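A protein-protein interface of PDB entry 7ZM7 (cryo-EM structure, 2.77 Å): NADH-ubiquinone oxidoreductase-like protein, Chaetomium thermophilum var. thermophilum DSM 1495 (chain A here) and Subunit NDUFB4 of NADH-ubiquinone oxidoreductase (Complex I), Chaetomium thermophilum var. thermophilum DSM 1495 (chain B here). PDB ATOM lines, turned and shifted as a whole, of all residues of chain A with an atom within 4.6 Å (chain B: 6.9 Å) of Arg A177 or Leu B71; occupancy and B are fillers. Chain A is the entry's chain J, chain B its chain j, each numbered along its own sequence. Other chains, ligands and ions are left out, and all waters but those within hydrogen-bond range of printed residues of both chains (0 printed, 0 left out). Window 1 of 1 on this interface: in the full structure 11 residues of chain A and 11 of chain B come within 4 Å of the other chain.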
ATOM      1  N   TYR A 173      -4.628  23.581  -1.872  1.00  0.00           N
ATOM      2  CA  TYR A 173      -3.291  23.810  -2.490  1.00  0.00           C
ATOM      3  C   TYR A 173      -2.416  24.655  -1.566  1.00  0.00           C
ATOM      4  O   TYR A 173      -1.211  24.379  -1.492  1.00  0.00           O
ATOM      5  CB  TYR A 173      -3.424  24.493  -3.854  1.00  0.00           C
ATOM      6  CG  TYR A 173      -2.149  24.931  -4.530  1.00  0.00           C
ATOM      7  CD1 TYR A 173      -1.379  24.040  -5.256  1.00  0.00           C
ATOM      8  CD2 TYR A 173      -1.732  26.250  -4.475  1.00  0.00           C
ATOM      9  CE1 TYR A 173      -0.214  24.441  -5.886  1.00  0.00           C
ATOM     10  CE2 TYR A 173      -0.569  26.668  -5.098  1.00  0.00           C
ATOM     11  CZ  TYR A 173       0.194  25.759  -5.804  1.00  0.00           C
ATOM     12  OH  TYR A 173       1.339  26.163  -6.424  1.00  0.00           O
ATOM     13  N   TYR A 174      -2.987  25.667  -0.913  1.00  0.00           N
ATOM     14  CA  TYR A 174      -2.190  26.587  -0.060  1.00  0.00           C
ATOM     15  C   TYR A 174      -1.566  25.856   1.137  1.00  0.00           C
ATOM     16  O   TYR A 174      -0.370  26.062   1.410  1.00  0.00           O
ATOM     17  CB  TYR A 174      -3.078  27.742   0.411  1.00  0.00           C
ATOM     18  CG  TYR A 174      -3.476  28.697  -0.684  1.00  0.00           C
ATOM     19  CD1 TYR A 174      -2.556  29.128  -1.624  1.00  0.00           C
ATOM     20  CD2 TYR A 174      -4.770  29.179  -0.779  1.00  0.00           C
ATOM     21  CE1 TYR A 174      -2.909  30.007  -2.634  1.00  0.00           C
ATOM     22  CE2 TYR A 174      -5.140  30.060  -1.779  1.00  0.00           C
ATOM     23  CZ  TYR A 174      -4.207  30.475  -2.712  1.00  0.00           C
ATOM     24  OH  TYR A 174      -4.570  31.343  -3.701  1.00  0.00           O
ATOM     25  N   GLU A 175      -2.351  25.031   1.827  1.00  0.00           N
ATOM     26  CA  GLU A 175      -1.845  24.295   3.013  1.00  0.00           C
ATOM     27  C   GLU A 175      -0.772  23.306   2.560  1.00  0.00           C
ATOM     28  O   GLU A 175       0.218  23.133   3.282  1.00  0.00           O
ATOM     29  CB  GLU A 175      -2.998  23.590   3.730  1.00  0.00           C
ATOM     30  N   ARG A 176      -0.999  22.644   1.433  1.00  0.00           N
ATOM     31  CA  ARG A 176       0.038  21.735   0.893  1.00  0.00           C
ATOM     32  C   ARG A 176       1.266  22.565   0.509  1.00  0.00           C
ATOM     33  O   ARG A 176       2.384  22.126   0.800  1.00  0.00           O
ATOM     34  CB  ARG A 176      -0.516  20.905  -0.265  1.00  0.00           C
ATOM     35  CG  ARG A 176      -1.629  19.944   0.119  1.00  0.00           C
ATOM     36  CD  ARG A 176      -1.956  18.983  -1.010  1.00  0.00           C
ATOM     37  NE  ARG A 176      -2.057  19.648  -2.302  1.00  0.00           N
ATOM     38  CZ  ARG A 176      -3.184  20.104  -2.838  1.00  0.00           C
ATOM     39  NH1 ARG A 176      -3.158  20.698  -4.019  1.00  0.00           N
ATOM     40  NH2 ARG A 176      -4.330  19.961  -2.199  1.00  0.00           N
ATOM     41  N   ARG A 177       1.054  23.726  -0.112  1.00  0.00           N
ATOM     42  CA  ARG A 177       2.194  24.543  -0.594  1.00  0.00           C
ATOM     43  C   ARG A 177       2.974  24.957   0.633  1.00  0.00           C
ATOM     44  O   ARG A 177       4.215  24.970   0.565  1.00  0.00           O
ATOM     45  CB  ARG A 177       1.722  25.758  -1.401  1.00  0.00           C
ATOM     46  CG  ARG A 177       2.837  26.529  -2.094  1.00  0.00           C
ATOM     47  CD  ARG A 177       2.308  27.744  -2.828  1.00  0.00           C
ATOM     48  NE  ARG A 177       2.517  28.954  -2.049  1.00  0.00           N
ATOM     49  CZ  ARG A 177       3.407  29.890  -2.342  1.00  0.00           C
ATOM     50  NH1 ARG A 177       3.534  30.949  -1.566  1.00  0.00           N
ATOM     51  NH2 ARG A 177       4.161  29.778  -3.418  1.00  0.00           N
ATOM     52  N   ALA A 178       2.258  25.290   1.705  1.00  0.00           N
ATOM     53  CA  ALA A 178       2.963  25.596   2.942  1.00  0.00           C
ATOM     54  C   ALA A 178       3.932  24.482   3.288  1.00  0.00           C
ATOM     55  O   ALA A 178       5.116  24.726   3.537  1.00  0.00           O
ATOM     56  CB  ALA A 178       1.962  25.807   4.075  1.00  0.00           C
ATOM     57  N   GLN A 179       3.455  23.241   3.249  1.00  0.00           N
ATOM     58  CA  GLN A 179       4.312  22.110   3.566  1.00  0.00           C
ATOM     59  C   GLN A 179       5.456  21.976   2.570  1.00  0.00           C
ATOM     60  O   GLN A 179       6.606  21.764   2.960  1.00  0.00           O
ATOM     61  CB  GLN A 179       3.481  20.831   3.604  1.00  0.00           C
ATOM     62  CG  GLN A 179       4.284  19.616   4.002  1.00  0.00           C
ATOM     63  CD  GLN A 179       4.761  19.710   5.431  1.00  0.00           C
ATOM     64  OE1 GLN A 179       4.023  20.143   6.315  1.00  0.00           O
ATOM     65  NE2 GLN A 179       6.007  19.321   5.664  1.00  0.00           N
ATOM     66  N   ARG A 180       5.159  22.094   1.283  1.00  0.00           N
ATOM     67  CA  ARG A 180       6.191  21.905   0.274  1.00  0.00           C
ATOM     68  C   ARG A 180       7.310  22.924   0.437  1.00  0.00           C
ATOM     69  O   ARG A 180       8.494  22.582   0.347  1.00  0.00           O
ATOM     70  CB  ARG A 180       5.565  22.005  -1.107  1.00  0.00           C
ATOM     71  CG  ARG A 180       6.420  21.509  -2.237  1.00  0.00           C
ATOM     72  CD  ARG A 180       5.576  21.318  -3.488  1.00  0.00           C
ATOM     73  NE  ARG A 180       5.090  22.586  -4.028  1.00  0.00           N
ATOM     74  CZ  ARG A 180       3.872  23.075  -3.818  1.00  0.00           C
ATOM     75  NH1 ARG A 180       3.522  24.231  -4.353  1.00  0.00           N
ATOM     76  NH2 ARG A 180       3.008  22.415  -3.062  1.00  0.00           N
ATOM     77  N   LEU A 181       6.951  24.184   0.686  1.00  0.00           N
ATOM     78  CA  LEU A 181       7.960  25.215   0.861  1.00  0.00           C
ATOM     79  C   LEU A 181       8.740  25.011   2.147  1.00  0.00           C
ATOM     80  O   LEU A 181       9.955  25.230   2.180  1.00  0.00           O
ATOM     81  CB  LEU A 181       7.305  26.592   0.842  1.00  0.00           C
ATOM     82  CG  LEU A 181       6.942  27.110  -0.547  1.00  0.00           C
ATOM     83  CD1 LEU A 181       6.385  28.514  -0.469  1.00  0.00           C
ATOM     84  CD2 LEU A 181       8.163  27.064  -1.445  1.00  0.00           C
ATOM     85  N   TYR A 185      12.621  25.044   1.251  1.00  0.00           N
ATOM     86  CA  TYR A 185      13.321  26.282   1.692  1.00  0.00           C
ATOM     87  C   TYR A 185      13.635  26.243   3.192  1.00  0.00           C
ATOM     88  O   TYR A 185      14.718  26.721   3.581  1.00  0.00           O
ATOM     89  CB  TYR A 185      12.558  27.530   1.237  1.00  0.00           C
ATOM     90  CG  TYR A 185      12.586  27.750  -0.254  1.00  0.00           C
ATOM     91  CD1 TYR A 185      11.441  27.612  -1.023  1.00  0.00           C
ATOM     92  CD2 TYR A 185      13.765  28.076  -0.904  1.00  0.00           C
ATOM     93  CE1 TYR A 185      11.465  27.807  -2.393  1.00  0.00           C
ATOM     94  CE2 TYR A 185      13.805  28.273  -2.273  1.00  0.00           C
ATOM     95  CZ  TYR A 185      12.651  28.139  -3.021  1.00  0.00           C
ATOM     96  OH  TYR A 185      12.686  28.332  -4.372  1.00  0.00           O
ATOM     97  N   ILE A 189       5.795  30.018   6.550  1.00  0.00           N
ATOM     98  CA  ILE A 189       4.999  31.005   5.831  1.00  0.00           C
ATOM     99  C   ILE A 189       4.077  31.722   6.803  1.00  0.00           C
ATOM    100  O   ILE A 189       3.327  31.088   7.554  1.00  0.00           O
ATOM    101  CB  ILE A 189       4.197  30.346   4.703  1.00  0.00           C
ATOM    102  CG1 ILE A 189       5.133  29.897   3.584  1.00  0.00           C
ATOM    103  CG2 ILE A 189       3.123  31.291   4.197  1.00  0.00           C
ATOM    104  CD1 ILE A 189       4.414  29.383   2.378  1.00  0.00           C
ATOM    105  N   LEU B  60       7.250  27.848 -11.711  1.00  0.00           N
ATOM    106  CA  LEU B  60       8.250  27.956 -10.619  1.00  0.00           C
ATOM    107  C   LEU B  60       7.871  29.164  -9.760  1.00  0.00           C
ATOM    108  O   LEU B  60       8.029  29.082  -8.534  1.00  0.00           O
ATOM    109  CB  LEU B  60       9.655  28.104 -11.206  1.00  0.00           C
ATOM    110  CG  LEU B  60      10.807  27.975 -10.212  1.00  0.00           C
ATOM    111  CD1 LEU B  60      10.600  26.783  -9.290  1.00  0.00           C
ATOM    112  CD2 LEU B  60      12.135  27.859 -10.941  1.00  0.00           C
ATOM    113  N   ASP B  62       5.049  32.605  -8.883  1.00  0.00           N
ATOM    114  CA  ASP B  62       3.756  33.315  -9.087  1.00  0.00           C
ATOM    115  C   ASP B  62       3.819  34.620  -8.283  1.00  0.00           C
ATOM    116  O   ASP B  62       4.228  34.557  -7.113  1.00  0.00           O
ATOM    117  CB  ASP B  62       2.564  32.450  -8.680  1.00  0.00           C
ATOM    118  CG  ASP B  62       1.216  33.110  -8.904  1.00  0.00           C
ATOM    119  OD1 ASP B  62       1.022  33.689  -9.987  1.00  0.00           O
ATOM    120  OD2 ASP B  62       0.372  33.038  -7.990  1.00  0.00           O
ATOM    121  N   LYS B  66       0.767  37.764  -3.762  1.00  0.00           N
ATOM    122  CA  LYS B  66       1.819  37.454  -2.802  1.00  0.00           C
ATOM    123  C   LYS B  66       2.205  38.689  -2.006  1.00  0.00           C
ATOM    124  O   LYS B  66       2.391  39.767  -2.567  1.00  0.00           O
ATOM    125  CB  LYS B  66       3.045  36.899  -3.521  1.00  0.00           C
ATOM    126  CG  LYS B  66       2.772  35.692  -4.373  1.00  0.00           C
ATOM    127  CD  LYS B  66       2.827  34.431  -3.540  1.00  0.00           C
ATOM    128  CE  LYS B  66       2.957  33.200  -4.399  1.00  0.00           C
ATOM    129  NZ  LYS B  66       1.849  33.095  -5.359  1.00  0.00           N
ATOM    130  N   ARG B  67       2.291  38.525  -0.687  1.00  0.00           N
ATOM    131  CA  ARG B  67       2.627  39.665   0.196  1.00  0.00           C
ATOM    132  C   ARG B  67       3.942  39.370   0.909  1.00  0.00           C
ATOM    133  O   ARG B  67       4.589  38.366   0.568  1.00  0.00           O
ATOM    134  CB  ARG B  67       1.538  39.853   1.251  1.00  0.00           C
ATOM    135  CG  ARG B  67       0.247  40.443   0.707  1.00  0.00           C
ATOM    136  CD  ARG B  67      -0.691  40.805   1.838  1.00  0.00           C
ATOM    137  NE  ARG B  67      -1.057  39.652   2.644  1.00  0.00           N
ATOM    138  CZ  ARG B  67      -2.162  38.939   2.474  1.00  0.00           C
ATOM    139  NH1 ARG B  67      -3.021  39.266   1.525  1.00  0.00           N
ATOM    140  NH2 ARG B  67      -2.409  37.905   3.259  1.00  0.00           N
ATOM    141  N   ARG B  68       4.324  40.231   1.852  1.00  0.00           N
ATOM    142  CA  ARG B  68       5.551  39.990   2.651  1.00  0.00           C
ATOM    143  C   ARG B  68       5.300  38.828   3.616  1.00  0.00           C
ATOM    144  O   ARG B  68       4.198  38.765   4.187  1.00  0.00           O
ATOM    145  CB  ARG B  68       5.977  41.279   3.352  1.00  0.00           C
ATOM    146  CG  ARG B  68       7.233  41.892   2.747  1.00  0.00           C
ATOM    147  CD  ARG B  68       7.712  43.159   3.424  1.00  0.00           C
ATOM    148  NE  ARG B  68       6.588  44.011   3.769  1.00  0.00           N
ATOM    149  CZ  ARG B  68       6.098  44.148   4.993  1.00  0.00           C
ATOM    150  NH1 ARG B  68       5.059  44.935   5.195  1.00  0.00           N
ATOM    151  NH2 ARG B  68       6.642  43.502   6.008  1.00  0.00           N
ATOM    152  N   GLY B  69       6.291  37.955   3.795  1.00  0.00           N
ATOM    153  CA  GLY B  69       6.114  36.775   4.659  1.00  0.00           C
ATOM    154  C   GLY B  69       5.733  35.570   3.828  1.00  0.00           C
ATOM    155  O   GLY B  69       5.845  34.442   4.339  1.00  0.00           O
ATOM    156  N   ASP B  70       5.291  35.806   2.590  1.00  0.00           N
ATOM    157  CA  ASP B  70       4.925  34.697   1.669  1.00  0.00           C
ATOM    158  C   ASP B  70       6.084  34.578   0.678  1.00  0.00           C
ATOM    159  O   ASP B  70       6.958  35.462   0.711  1.00  0.00           O
ATOM    160  CB  ASP B  70       3.600  34.981   0.961  1.00  0.00           C
ATOM    161  CG  ASP B  70       2.880  33.731   0.488  1.00  0.00           C
ATOM    162  OD1 ASP B  70       3.335  32.626   0.839  1.00  0.00           O
ATOM    163  OD2 ASP B  70       1.870  33.873  -0.228  1.00  0.00           O
ATOM    164  N   LEU B  71       6.116  33.530  -0.144  1.00  0.00           N
ATOM    165  CA  LEU B  71       7.281  33.357  -1.053  1.00  0.00           C
ATOM    166  C   LEU B  71       6.802  33.370  -2.507  1.00  0.00           C
ATOM    167  O   LEU B  71       5.743  32.784  -2.778  1.00  0.00           O
ATOM    168  CB  LEU B  71       7.995  32.044  -0.718  1.00  0.00           C
ATOM    169  CG  LEU B  71       9.061  32.139   0.372  1.00  0.00           C
ATOM    170  CD1 LEU B  71       9.801  30.819   0.520  1.00  0.00           C
ATOM    171  CD2 LEU B  71      10.041  33.261   0.067  1.00  0.00           C
ATOM    172  N   ILE B  72       7.554  34.022  -3.397  1.00  0.00           N
ATOM    173  CA  ILE B  72       7.195  34.057  -4.847  1.00  0.00           C
ATOM    174  C   ILE B  72       7.233  32.626  -5.377  1.00  0.00           C
ATOM    175  O   ILE B  72       6.331  32.256  -6.151  1.00  0.00           O
ATOM    176  CB  ILE B  72       8.172  34.954  -5.633  1.00  0.00           C
ATOM    177  CG1 ILE B  72       8.199  36.388  -5.104  1.00  0.00           C
ATOM    178  CG2 ILE B  72       7.879  34.910  -7.123  1.00  0.00           C
ATOM    179  CD1 ILE B  72       9.173  37.279  -5.834  1.00  0.00           C
ATOM    180  N   SER B  73       8.226  31.844  -4.950  1.00  0.00           N
ATOM    181  CA  SER B  73       8.381  30.469  -5.488  1.00  0.00           C
ATOM    182  C   SER B  73       7.142  29.637  -5.160  1.00  0.00           C
ATOM    183  O   SER B  73       6.674  29.695  -4.008  1.00  0.00           O
ATOM    184  CB  SER B  73       9.629  29.827  -4.963  1.00  0.00           C
ATOM    185  OG  SER B  73      10.780  30.536  -5.394  1.00  0.00           O
ATOM    186  N   GLU B  74       6.645  28.886  -6.141  1.00  0.00           N
ATOM    187  CA  GLU B  74       5.426  28.064  -5.946  1.00  0.00           C
ATOM    188  C   GLU B  74       5.822  26.593  -5.841  1.00  0.00           C
ATOM    189  O   GLU B  74       4.916  25.759  -5.663  1.00  0.00           O
ATOM    190  CB  GLU B  74       4.469  28.273  -7.120  1.00  0.00           C
ATOM    191  CG  GLU B  74       3.272  29.140  -6.782  1.00  0.00           C
ATOM    192  CD  GLU B  74       2.194  29.138  -7.851  1.00  0.00           C
ATOM    193  OE1 GLU B  74       2.486  28.696  -8.980  1.00  0.00           O
ATOM    194  OE2 GLU B  74       1.064  29.575  -7.551  1.00  0.00           O
ATOM    195  N   ARG B  75       7.120  26.289  -5.948  1.00  0.00           N
ATOM    196  CA  ARG B  75       7.543  24.900  -5.983  1.00  0.00           C
ATOM    197  C   ARG B  75       8.930  24.733  -5.382  1.00  0.00           C
ATOM    198  O   ARG B  75       9.249  23.704  -4.788  1.00  0.00           O
ATOM    199  CB  ARG B  75       7.522  24.379  -7.421  1.00  0.00           C
ATOM    200  CG  ARG B  75       8.030  22.962  -7.576  1.00  0.00           C
ATOM    201  CD  ARG B  75       7.850  22.453  -8.992  1.00  0.00           C
ATOM    202  NE  ARG B  75       8.697  23.125  -9.972  1.00  0.00           N
ATOM    203  CZ  ARG B  75       8.257  24.021 -10.846  1.00  0.00           C
ATOM    204  NH1 ARG B  75       9.083  24.566 -11.722  1.00  0.00           N
ATOM    205  NH2 ARG B  75       6.985  24.363 -10.850  1.00  0.00           N
ATOM    206  OXT ARG B  75       9.765  25.629  -5.472  1.00  0.00           O
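The side-chain carboxylate of Asp B70 lies within salt-bridge range of the guanidinium group of Arg A177 (2.9 Å).
NH1 of Arg A177 is in hydrogen-bond range of O of Leu B71, 3.1 Å away.
The guanidinium group (NH2) of Arg A177 lies within hydrogen-bond range of the backbone carbonyl oxygen (O) of Ser B73, at 2.6 Å.
The guanidinium group (NH1) of Arg A180 lies within hydrogen-bond range of the backbone carbonyl oxygen (O) of Glu B74, 2.4 Å away.
OG of Ser B73 sits at hydrogen-bond distance from OH of Tyr A185 (3.1 Å).
OH of Tyr A173 touches CD of Glu B74, 3.4 Å away.
Arg A177 touches Lys B66 (NH1 to CE, 3.7 Å).
Arg A177 touches Glu B74 (NH2 to CA, 3.3 Å).
Arg B75 touches Arg A180.
Leu B71 touches Leu A181 (CB to CD1, 3.9 Å).
CD1 of Leu A181 touches O of Ser B73, 3.7 Å away.
Leu B71 touches Tyr A185.
Ile A189 touches Gly B69.
Asp B70 touches Ile A189 (OD1 to CG2, 3.6 Å).
O of Leu B60 sits at hydrogen-bond distance from N of Glu B74 (2.8 Å).
The side-chain amino group (NZ) of Lys B66 is in salt-bridge range of the side-chain carboxylate (OD2) of Asp B62, 3.0 Å away.
Hydrophobic or aromatic side chains of chain B that line the printed part of chain A: Leu B71.
Hydrophobic or aromatic side chains of chain A within 4 Å of the printed part of chain B: Tyr A173, Leu A181, Tyr A185 and Ile A189.
Along chain A the printed residues that touch a printed residue of chain B span positions 173 to 189.
Among the printed residues, 14 pairs touch across the chains.
Among the printed residues, Asp or Glu carboxylates within 4 Å of a Lys or Arg side-chain nitrogen of the other chain: Arg A177 with Asp B70 (2.9 Å).
Gln A179 touches none of the printed residues of chain B.
Printed residues of chain B within 4 Å of Leu A181: Leu B71 (3.9 Å) and Ser B73 (3.7 Å).
Of the printed residues of chain B, Ile A189 touches Gly B69 and Asp B70.
Arg B67 touches none of the printed residues of chain A.
Of the printed residues of chain A, Gly B69 touches Ile A189.
Of the printed residues of chain A, Asp B70 touches Arg A177 (2.9 Å) and Ile A189 (3.6 Å).
Of chain A, only Arg A177, Leu A181 and Tyr A185 come within 4 Å of Leu B71.
Of the printed residues of chain A, Ser B73 touches Arg A177 (2.6 Å), Leu A181 (3.7 Å) and Tyr A185 (3.1 Å).
The nearest residue of chain B that does not touch Arg A177 is Ile B72 (4.3 Å).
The nearest printed residue of chain A that does not touch Leu B71 is Ile A189 (5.1 Å).
The nearest printed residue of chain B that does not touch Tyr A173 is Arg B75 (5.8 Å).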
